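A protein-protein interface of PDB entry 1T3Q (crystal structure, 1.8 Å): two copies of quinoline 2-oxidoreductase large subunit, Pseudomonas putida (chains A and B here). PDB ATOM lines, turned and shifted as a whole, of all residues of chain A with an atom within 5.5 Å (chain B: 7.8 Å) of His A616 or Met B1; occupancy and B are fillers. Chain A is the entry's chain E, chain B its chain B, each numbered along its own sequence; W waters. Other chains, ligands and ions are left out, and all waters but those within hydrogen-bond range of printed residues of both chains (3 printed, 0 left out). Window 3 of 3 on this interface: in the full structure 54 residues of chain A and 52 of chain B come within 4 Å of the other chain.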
ATOM      1  N   LEU A 571     -15.418 -16.891 -16.331  1.00  0.00           N
ATOM      2  CA  LEU A 571     -15.720 -17.583 -15.088  1.00  0.00           C
ATOM      3  C   LEU A 571     -17.042 -18.336 -15.213  1.00  0.00           C
ATOM      4  O   LEU A 571     -17.155 -19.482 -14.784  1.00  0.00           O
ATOM      5  CB  LEU A 571     -15.798 -16.588 -13.928  1.00  0.00           C
ATOM      6  CG  LEU A 571     -16.074 -17.188 -12.546  1.00  0.00           C
ATOM      7  CD1 LEU A 571     -15.011 -18.225 -12.216  1.00  0.00           C
ATOM      8  CD2 LEU A 571     -16.083 -16.083 -11.501  1.00  0.00           C
ATOM      9  N   HIS A 574     -16.640 -21.451 -17.302  1.00  0.00           N
ATOM     10  CA  HIS A 574     -15.996 -22.504 -16.531  1.00  0.00           C
ATOM     11  C   HIS A 574     -17.014 -23.195 -15.625  1.00  0.00           C
ATOM     12  O   HIS A 574     -17.076 -24.422 -15.567  1.00  0.00           O
ATOM     13  CB  HIS A 574     -14.873 -21.901 -15.683  1.00  0.00           C
ATOM     14  CG  HIS A 574     -14.057 -22.914 -14.945  1.00  0.00           C
ATOM     15  ND1 HIS A 574     -13.186 -23.774 -15.579  1.00  0.00           N
ATOM     16  CD2 HIS A 574     -13.973 -23.198 -13.624  1.00  0.00           C
ATOM     17  CE1 HIS A 574     -12.599 -24.543 -14.680  1.00  0.00           C
ATOM     18  NE2 HIS A 574     -13.059 -24.215 -13.486  1.00  0.00           N
ATOM     19  N   ALA A 608     -18.156 -15.042  -6.795  1.00  0.00           N
ATOM     20  CA  ALA A 608     -17.182 -16.119  -6.911  1.00  0.00           C
ATOM     21  C   ALA A 608     -15.868 -15.566  -7.462  1.00  0.00           C
ATOM     22  O   ALA A 608     -14.782 -15.985  -7.056  1.00  0.00           O
ATOM     23  CB  ALA A 608     -17.718 -17.215  -7.829  1.00  0.00           C
ATOM     24  N   ALA A 609     -15.973 -14.628  -8.393  1.00  0.00           N
ATOM     25  CA  ALA A 609     -14.786 -14.020  -8.985  1.00  0.00           C
ATOM     26  C   ALA A 609     -13.944 -13.382  -7.882  1.00  0.00           C
ATOM     27  O   ALA A 609     -12.717 -13.504  -7.870  1.00  0.00           O
ATOM     28  CB  ALA A 609     -15.192 -12.969 -10.010  1.00  0.00           C
ATOM     29  N   TYR A 610     -14.613 -12.703  -6.954  1.00  0.00           N
ATOM     30  CA  TYR A 610     -13.927 -12.044  -5.847  1.00  0.00           C
ATOM     31  C   TYR A 610     -13.518 -12.961  -4.702  1.00  0.00           C
ATOM     32  O   TYR A 610     -12.380 -12.916  -4.236  1.00  0.00           O
ATOM     33  CB  TYR A 610     -14.808 -10.936  -5.237  1.00  0.00           C
ATOM     34  CG  TYR A 610     -14.720  -9.592  -5.920  1.00  0.00           C
ATOM     35  CD1 TYR A 610     -15.541  -9.280  -6.999  1.00  0.00           C
ATOM     36  CD2 TYR A 610     -13.794  -8.637  -5.495  1.00  0.00           C
ATOM     37  CE1 TYR A 610     -15.444  -8.049  -7.644  1.00  0.00           C
ATOM     38  CE2 TYR A 610     -13.686  -7.404  -6.132  1.00  0.00           C
ATOM     39  CZ  TYR A 610     -14.510  -7.116  -7.206  1.00  0.00           C
ATOM     40  OH  TYR A 610     -14.384  -5.913  -7.860  1.00  0.00           O
ATOM     41  N   ALA A 612     -14.264 -16.716  -4.401  1.00  0.00           N
ATOM     42  CA  ALA A 612     -14.267 -18.175  -4.548  1.00  0.00           C
ATOM     43  C   ALA A 612     -13.167 -18.648  -5.495  1.00  0.00           C
ATOM     44  O   ALA A 612     -13.423 -19.112  -6.609  1.00  0.00           O
ATOM     45  CB  ALA A 612     -15.636 -18.651  -5.034  1.00  0.00           C
ATOM     46  N   ASP A 613     -11.939 -18.515  -5.007  1.00  0.00           N
ATOM     47  CA  ASP A 613     -10.703 -18.879  -5.688  1.00  0.00           C
ATOM     48  C   ASP A 613     -10.720 -20.266  -6.347  1.00  0.00           C
ATOM     49  O   ASP A 613     -10.115 -20.465  -7.401  1.00  0.00           O
ATOM     50  CB  ASP A 613      -9.574 -18.768  -4.650  1.00  0.00           C
ATOM     51  CG  ASP A 613      -8.264 -19.313  -5.129  1.00  0.00           C
ATOM     52  OD1 ASP A 613      -8.135 -20.551  -5.218  1.00  0.00           O
ATOM     53  OD2 ASP A 613      -7.354 -18.504  -5.401  1.00  0.00           O
ATOM     54  N   ALA A 614     -11.414 -21.217  -5.730  1.00  0.00           N
ATOM     55  CA  ALA A 614     -11.484 -22.576  -6.265  1.00  0.00           C
ATOM     56  C   ALA A 614     -12.310 -22.710  -7.542  1.00  0.00           C
ATOM     57  O   ALA A 614     -12.151 -23.677  -8.283  1.00  0.00           O
ATOM     58  CB  ALA A 614     -12.021 -23.526  -5.200  1.00  0.00           C
ATOM     59  N   THR A 615     -13.183 -21.743  -7.803  1.00  0.00           N
ATOM     60  CA  THR A 615     -14.030 -21.775  -8.995  1.00  0.00           C
ATOM     61  C   THR A 615     -13.364 -21.148 -10.215  1.00  0.00           C
ATOM     62  O   THR A 615     -13.900 -21.221 -11.324  1.00  0.00           O
ATOM     63  CB  THR A 615     -15.357 -21.021  -8.766  1.00  0.00           C
ATOM     64  OG1 THR A 615     -15.087 -19.621  -8.599  1.00  0.00           O
ATOM     65  CG2 THR A 615     -16.059 -21.543  -7.532  1.00  0.00           C
ATOM     66  N   HIS A 616     -12.201 -20.534 -10.018  1.00  0.00           N
ATOM     67  CA  HIS A 616     -11.503 -19.876 -11.116  1.00  0.00           C
ATOM     68  C   HIS A 616     -10.853 -20.835 -12.108  1.00  0.00           C
ATOM     69  O   HIS A 616     -10.239 -21.826 -11.718  1.00  0.00           O
ATOM     70  CB  HIS A 616     -10.427 -18.929 -10.569  1.00  0.00           C
ATOM     71  CG  HIS A 616     -10.963 -17.830  -9.706  1.00  0.00           C
ATOM     72  ND1 HIS A 616     -12.296 -17.728  -9.372  1.00  0.00           N
ATOM     73  CD2 HIS A 616     -10.342 -16.794  -9.099  1.00  0.00           C
ATOM     74  CE1 HIS A 616     -12.473 -16.674  -8.595  1.00  0.00           C
ATOM     75  NE2 HIS A 616     -11.302 -16.090  -8.414  1.00  0.00           N
ATOM     76  N   PRO A 617     -10.993 -20.550 -13.411  1.00  0.00           N
ATOM     77  CA  PRO A 617     -10.405 -21.390 -14.457  1.00  0.00           C
ATOM     78  C   PRO A 617      -8.904 -21.105 -14.544  1.00  0.00           C
ATOM     79  O   PRO A 617      -8.446 -20.024 -14.170  1.00  0.00           O
ATOM     80  CB  PRO A 617     -11.156 -20.951 -15.711  1.00  0.00           C
ATOM     81  CG  PRO A 617     -11.439 -19.504 -15.437  1.00  0.00           C
ATOM     82  CD  PRO A 617     -11.887 -19.534 -13.995  1.00  0.00           C
ATOM     83  N   PRO A 618      -8.116 -22.069 -15.044  1.00  0.00           N
ATOM     84  CA  PRO A 618      -6.670 -21.854 -15.150  1.00  0.00           C
ATOM     85  C   PRO A 618      -6.285 -20.618 -15.965  1.00  0.00           C
ATOM     86  O   PRO A 618      -6.873 -20.343 -17.014  1.00  0.00           O
ATOM     87  CB  PRO A 618      -6.173 -23.161 -15.778  1.00  0.00           C
ATOM     88  CG  PRO A 618      -7.354 -23.623 -16.583  1.00  0.00           C
ATOM     89  CD  PRO A 618      -8.510 -23.351 -15.652  1.00  0.00           C
ATOM     90  N   GLY A 619      -5.304 -19.871 -15.462  1.00  0.00           N
ATOM     91  CA  GLY A 619      -4.840 -18.673 -16.148  1.00  0.00           C
ATOM     92  C   GLY A 619      -5.748 -17.461 -16.012  1.00  0.00           C
ATOM     93  O   GLY A 619      -5.510 -16.422 -16.627  1.00  0.00           O
ATOM     94  N   PHE A 620      -6.787 -17.595 -15.199  1.00  0.00           N
ATOM     95  CA  PHE A 620      -7.760 -16.524 -14.975  1.00  0.00           C
ATOM     96  C   PHE A 620      -7.160 -15.281 -14.324  1.00  0.00           C
ATOM     97  O   PHE A 620      -6.250 -15.379 -13.504  1.00  0.00           O
ATOM     98  CB  PHE A 620      -8.878 -17.055 -14.076  1.00  0.00           C
ATOM     99  CG  PHE A 620     -10.046 -16.120 -13.914  1.00  0.00           C
ATOM    100  CD1 PHE A 620     -10.469 -15.737 -12.643  1.00  0.00           C
ATOM    101  CD2 PHE A 620     -10.770 -15.681 -15.022  1.00  0.00           C
ATOM    102  CE1 PHE A 620     -11.599 -14.936 -12.474  1.00  0.00           C
ATOM    103  CE2 PHE A 620     -11.904 -14.879 -14.864  1.00  0.00           C
ATOM    104  CZ  PHE A 620     -12.319 -14.508 -13.587  1.00  0.00           C
ATOM    105  N   ALA A 622      -8.537 -12.517 -12.086  1.00  0.00           N
ATOM    106  CA  ALA A 622      -9.714 -12.160 -11.298  1.00  0.00           C
ATOM    107  C   ALA A 622      -9.972 -10.670 -11.105  1.00  0.00           C
ATOM    108  O   ALA A 622     -10.912 -10.287 -10.412  1.00  0.00           O
ATOM    109  CB  ALA A 622      -9.649 -12.855  -9.944  1.00  0.00           C
ATOM    110  N   MET B   1      -2.699 -18.785 -12.466  1.00  0.00           N
ATOM    111  CA  MET B   1      -3.600 -17.617 -12.257  1.00  0.00           C
ATOM    112  C   MET B   1      -2.803 -16.329 -12.435  1.00  0.00           C
ATOM    113  O   MET B   1      -1.690 -16.211 -11.931  1.00  0.00           O
ATOM    114  CB  MET B   1      -4.198 -17.667 -10.851  1.00  0.00           C
ATOM    115  CG  MET B   1      -5.031 -18.910 -10.582  1.00  0.00           C
ATOM    116  SD  MET B   1      -6.429 -19.048 -11.715  1.00  0.00           S
ATOM    117  CE  MET B   1      -7.195 -20.563 -11.107  1.00  0.00           C
ATOM    118  N   MET B   2      -3.373 -15.369 -13.152  1.00  0.00           N
ATOM    119  CA  MET B   2      -2.689 -14.103 -13.388  1.00  0.00           C
ATOM    120  C   MET B   2      -2.364 -13.337 -12.105  1.00  0.00           C
ATOM    121  O   MET B   2      -1.377 -12.603 -12.047  1.00  0.00           O
ATOM    122  CB  MET B   2      -3.520 -13.219 -14.322  1.00  0.00           C
ATOM    123  CG  MET B   2      -3.587 -13.728 -15.759  1.00  0.00           C
ATOM    124  SD  MET B   2      -1.946 -14.093 -16.416  1.00  0.00           S
ATOM    125  CE  MET B   2      -1.187 -12.456 -16.398  1.00  0.00           C
ATOM    126  N   LYS B   3      -3.182 -13.516 -11.072  1.00  0.00           N
ATOM    127  CA  LYS B   3      -2.955 -12.815  -9.809  1.00  0.00           C
ATOM    128  C   LYS B   3      -1.669 -13.273  -9.123  1.00  0.00           C
ATOM    129  O   LYS B   3      -1.165 -12.599  -8.225  1.00  0.00           O
ATOM    130  CB  LYS B   3      -4.146 -13.014  -8.861  1.00  0.00           C
ATOM    131  CG  LYS B   3      -4.357 -14.446  -8.400  1.00  0.00           C
ATOM    132  CD  LYS B   3      -5.560 -14.550  -7.472  1.00  0.00           C
ATOM    133  CE  LYS B   3      -5.707 -15.949  -6.907  1.00  0.00           C
ATOM    134  NZ  LYS B   3      -6.786 -16.009  -5.883  1.00  0.00           N
ATOM    135  N   HIS B   4      -1.136 -14.414  -9.557  1.00  0.00           N
ATOM    136  CA  HIS B   4       0.097 -14.965  -8.984  1.00  0.00           C
ATOM    137  C   HIS B   4       1.351 -14.323  -9.565  1.00  0.00           C
ATOM    138  O   HIS B   4       2.442 -14.453  -9.001  1.00  0.00           O
ATOM    139  CB  HIS B   4       0.174 -16.473  -9.247  1.00  0.00           C
ATOM    140  CG  HIS B   4      -0.826 -17.276  -8.479  1.00  0.00           C
ATOM    141  ND1 HIS B   4      -1.126 -18.584  -8.795  1.00  0.00           N
ATOM    142  CD2 HIS B   4      -1.572 -16.971  -7.391  1.00  0.00           C
ATOM    143  CE1 HIS B   4      -2.015 -19.050  -7.936  1.00  0.00           C
ATOM    144  NE2 HIS B   4      -2.304 -18.091  -7.074  1.00  0.00           N
ATOM    145  N   GLU B   5       1.189 -13.645 -10.695  1.00  0.00           N
ATOM    146  CA  GLU B   5       2.300 -13.012 -11.396  1.00  0.00           C
ATOM    147  C   GLU B   5       3.267 -12.228 -10.518  1.00  0.00           C
ATOM    148  O   GLU B   5       2.856 -11.424  -9.680  1.00  0.00           O
ATOM    149  CB  GLU B   5       1.775 -12.080 -12.496  1.00  0.00           C
ATOM    150  CG  GLU B   5       2.879 -11.546 -13.400  1.00  0.00           C
ATOM    151  CD  GLU B   5       2.414 -10.450 -14.343  1.00  0.00           C
ATOM    152  OE1 GLU B   5       3.165 -10.143 -15.294  1.00  0.00           O
ATOM    153  OE2 GLU B   5       1.314  -9.887 -14.134  1.00  0.00           O
ATOM    154  N   VAL B   6       4.560 -12.462 -10.737  1.00  0.00           N
ATOM    155  CA  VAL B   6       5.616 -11.771 -10.006  1.00  0.00           C
ATOM    156  C   VAL B   6       6.362 -10.943 -11.042  1.00  0.00           C
ATOM    157  O   VAL B   6       7.189 -11.468 -11.781  1.00  0.00           O
ATOM    158  CB  VAL B   6       6.604 -12.769  -9.359  1.00  0.00           C
ATOM    159  CG1 VAL B   6       7.678 -12.017  -8.581  1.00  0.00           C
ATOM    160  CG2 VAL B   6       5.851 -13.728  -8.454  1.00  0.00           C
ATOM    161  N   THR B 482     -10.734 -16.526   0.316  1.00  0.00           N
ATOM    162  CA  THR B 482     -10.098 -16.054  -0.908  1.00  0.00           C
ATOM    163  C   THR B 482      -9.920 -14.546  -0.746  1.00  0.00           C
ATOM    164  O   THR B 482     -10.858 -13.843  -0.380  1.00  0.00           O
ATOM    165  CB  THR B 482     -10.977 -16.315  -2.149  1.00  0.00           C
ATOM    166  OG1 THR B 482     -10.953 -17.711  -2.467  1.00  0.00           O
ATOM    167  CG2 THR B 482     -10.467 -15.523  -3.348  1.00  0.00           C
ATOM    168  N   THR B 483      -8.719 -14.045  -1.003  1.00  0.00           N
ATOM    169  CA  THR B 483      -8.488 -12.613  -0.877  1.00  0.00           C
ATOM    170  C   THR B 483      -8.515 -11.956  -2.246  1.00  0.00           C
ATOM    171  O   THR B 483      -8.448 -12.632  -3.266  1.00  0.00           O
ATOM    172  CB  THR B 483      -7.128 -12.310  -0.213  1.00  0.00           C
ATOM    173  OG1 THR B 483      -6.083 -12.981  -0.931  1.00  0.00           O
ATOM    174  CG2 THR B 483      -7.135 -12.776   1.239  1.00  0.00           C
ATOM    175  N   HIS B 484      -8.625 -10.631  -2.256  1.00  0.00           N
ATOM    176  CA  HIS B 484      -8.643  -9.862  -3.491  1.00  0.00           C
ATOM    177  C   HIS B 484      -7.993  -8.528  -3.144  1.00  0.00           C
ATOM    178  O   HIS B 484      -8.430  -7.845  -2.219  1.00  0.00           O
ATOM    179  CB  HIS B 484     -10.087  -9.663  -3.968  1.00  0.00           C
ATOM    180  CG  HIS B 484     -10.201  -9.122  -5.360  1.00  0.00           C
ATOM    181  ND1 HIS B 484      -9.986  -7.795  -5.668  1.00  0.00           N
ATOM    182  CD2 HIS B 484     -10.512  -9.733  -6.528  1.00  0.00           C
ATOM    183  CE1 HIS B 484     -10.162  -7.612  -6.964  1.00  0.00           C
ATOM    184  NE2 HIS B 484     -10.482  -8.772  -7.509  1.00  0.00           N
ATOM    185  N   ARG B 559       2.038  -5.712 -10.691  1.00  0.00           N
ATOM    186  CA  ARG B 559       1.218  -6.143 -11.820  1.00  0.00           C
ATOM    187  C   ARG B 559       0.626  -4.978 -12.612  1.00  0.00           C
ATOM    188  O   ARG B 559       0.710  -4.948 -13.838  1.00  0.00           O
ATOM    189  CB  ARG B 559       0.061  -7.028 -11.341  1.00  0.00           C
ATOM    190  CG  ARG B 559       0.424  -8.450 -10.937  1.00  0.00           C
ATOM    191  CD  ARG B 559      -0.812  -9.348 -11.094  1.00  0.00           C
ATOM    192  NE  ARG B 559      -1.238  -9.387 -12.493  1.00  0.00           N
ATOM    193  CZ  ARG B 559      -2.484  -9.599 -12.913  1.00  0.00           C
ATOM    194  NH1 ARG B 559      -2.741  -9.611 -14.214  1.00  0.00           N
ATOM    195  NH2 ARG B 559      -3.477  -9.779 -12.051  1.00  0.00           N
ATOM    196  N   THR B 629      -5.167  -7.320  -9.643  1.00  0.00           N
ATOM    197  CA  THR B 629      -5.164  -7.860  -8.302  1.00  0.00           C
ATOM    198  C   THR B 629      -3.972  -8.801  -8.193  1.00  0.00           C
ATOM    199  O   THR B 629      -3.490  -9.328  -9.204  1.00  0.00           O
ATOM    200  CB  THR B 629      -6.450  -8.647  -7.993  1.00  0.00           C
ATOM    201  OG1 THR B 629      -6.405  -9.098  -6.635  1.00  0.00           O
ATOM    202  CG2 THR B 629      -6.574  -9.855  -8.921  1.00  0.00           C
ATOM    203  N   ASP B 631      -2.134 -11.972  -5.539  1.00  0.00           N
ATOM    204  CA  ASP B 631      -2.285 -12.914  -4.443  1.00  0.00           C
ATOM    205  C   ASP B 631      -1.108 -13.881  -4.587  1.00  0.00           C
ATOM    206  O   ASP B 631      -0.969 -14.537  -5.610  1.00  0.00           O
ATOM    207  CB  ASP B 631      -3.632 -13.638  -4.610  1.00  0.00           C
ATOM    208  CG  ASP B 631      -4.021 -14.469  -3.400  1.00  0.00           C
ATOM    209  OD1 ASP B 631      -3.482 -14.233  -2.299  1.00  0.00           O
ATOM    210  OD2 ASP B 631      -4.892 -15.354  -3.554  1.00  0.00           O
ATOM    211  N   SER B 633       1.326 -17.017  -4.751  1.00  0.00           N
ATOM    212  CA  SER B 633       1.044 -18.395  -5.136  1.00  0.00           C
ATOM    213  C   SER B 633       1.323 -19.405  -4.031  1.00  0.00           C
ATOM    214  O   SER B 633       0.969 -20.580  -4.151  1.00  0.00           O
ATOM    215  CB  SER B 633       1.868 -18.755  -6.371  1.00  0.00           C
ATOM    216  OG  SER B 633       3.250 -18.614  -6.102  1.00  0.00           O
HETATM  217  O   HOH W   1      -3.067 -16.587 -18.327  1.00  0.00           O
HETATM  218  O   HOH W   2      -6.390 -14.370 -11.056  1.00  0.00           O
HETATM  219  O   HOH W   3      -3.779 -21.077 -13.265  1.00  0.00           O
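Water W2 lies within hydrogen-bond range of O of Phe A620 (2.7 Å), N of Ala A622 (3.0 Å) and N of Lys B3 (3.3 Å). Water W3 bridges N of Met B1 (2.7 Å) and N of Gly A619 (2.9 Å). Water W1 lies within hydrogen-bond range of the backbone carbonyl oxygen (O) of Gly A619 (3.0 Å) and the side-chain sulfur (SD) of Met B2 (3.3 Å).
Tyr A610 touches Thr B482 (O to CG2, 3.4 Å). His B484 touches Tyr A610 (CD2 to CD2, 3.6 Å). Ala A612 touches Thr B482. CE of Met B1 touches O of His A616 (3.4 Å). Gly A619 touches Met B1 (N to SD, 3.998 Å). Met B2 touches Gly A619.
The backbone carbonyl oxygen (O) of Ala A622 sits at hydrogen-bond distance from a ring nitrogen (NE2) of His B484 (3.3 Å). OG1 of Thr B482 lies close to N of Asp A613 (2.8 Å). The backbone NH (N) of Met B2 is in hydrogen-bond range of the backbone carbonyl oxygen (O) of Phe A620 (2.9 Å). The side-chain amino group (NZ) of Lys B3 lies within salt-bridge range of the side-chain carboxylate (OD2) of Asp A613 (2.6 Å). The backbone carbonyl oxygen (O) of Pro A617 lies close to the side-chain sulfur (SD) of Met B1. N of Phe A620 sits at hydrogen-bond distance from SD of Met B1, 3.8 Å away.
Of the 15 printed residues of chain A, 8 touch a printed residue of chain B. Along chain A the printed residues that touch a printed residue of chain B span positions 610 to 622. Of the 13 printed residues of chain B, 5 touch a printed residue of chain A. Among the printed residues, 12 pairs touch across the chains.
No position is printed for both chains.
Printed residues of chain B within 4 Å of Tyr A610: Thr B482 (3.4 Å) and His B484 (3.6 Å). Printed residues of chain B within 4 Å of Asp A613: Lys B3 and Thr B482. Of the printed residues of chain B, His A616 touches Met B1. Pro A617 touches one residue of chain B. Pro A618 touches none of the printed residues of chain B. Of the printed residues of chain B, Gly A619 touches Met B1 (3.998 Å) and Met B2 (3.4 Å). Printed residues of chain A within 4 Å of Met B1: His A616 (3.4 Å), Pro A617 (3.3 Å), Gly A619 (3.998 Å) and Phe A620 (3.7 Å). Of the printed residues of chain A, Lys B3 touches Asp A613 (2.6 Å). Thr B629 touches none of the printed residues of chain A.
The side-chain hydroxyl (OG1) of Thr A615 sits at hydrogen-bond distance from a ring nitrogen (ND1) of His A616 (3.5 Å). The backbone carbonyl oxygen (O) of Ala A612 sits close to a ring nitrogen (ND1) of His A616, at 3.3 Å. NZ of Lys B3 lies within salt-bridge range of OD2 of Asp B631 (3.1 Å). The backbone carbonyl oxygen of Ala A609 is in hydrogen-bond range of a ring nitrogen (NE2) of His A616. The backbone carbonyl oxygen (O) of Met B2 sits at hydrogen-bond distance from the guanidinium group (NE) of Arg B559, at 3.2 Å. O of Ala A612 is in hydrogen-bond range of OG1 of Thr A615, at 2.6 Å.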
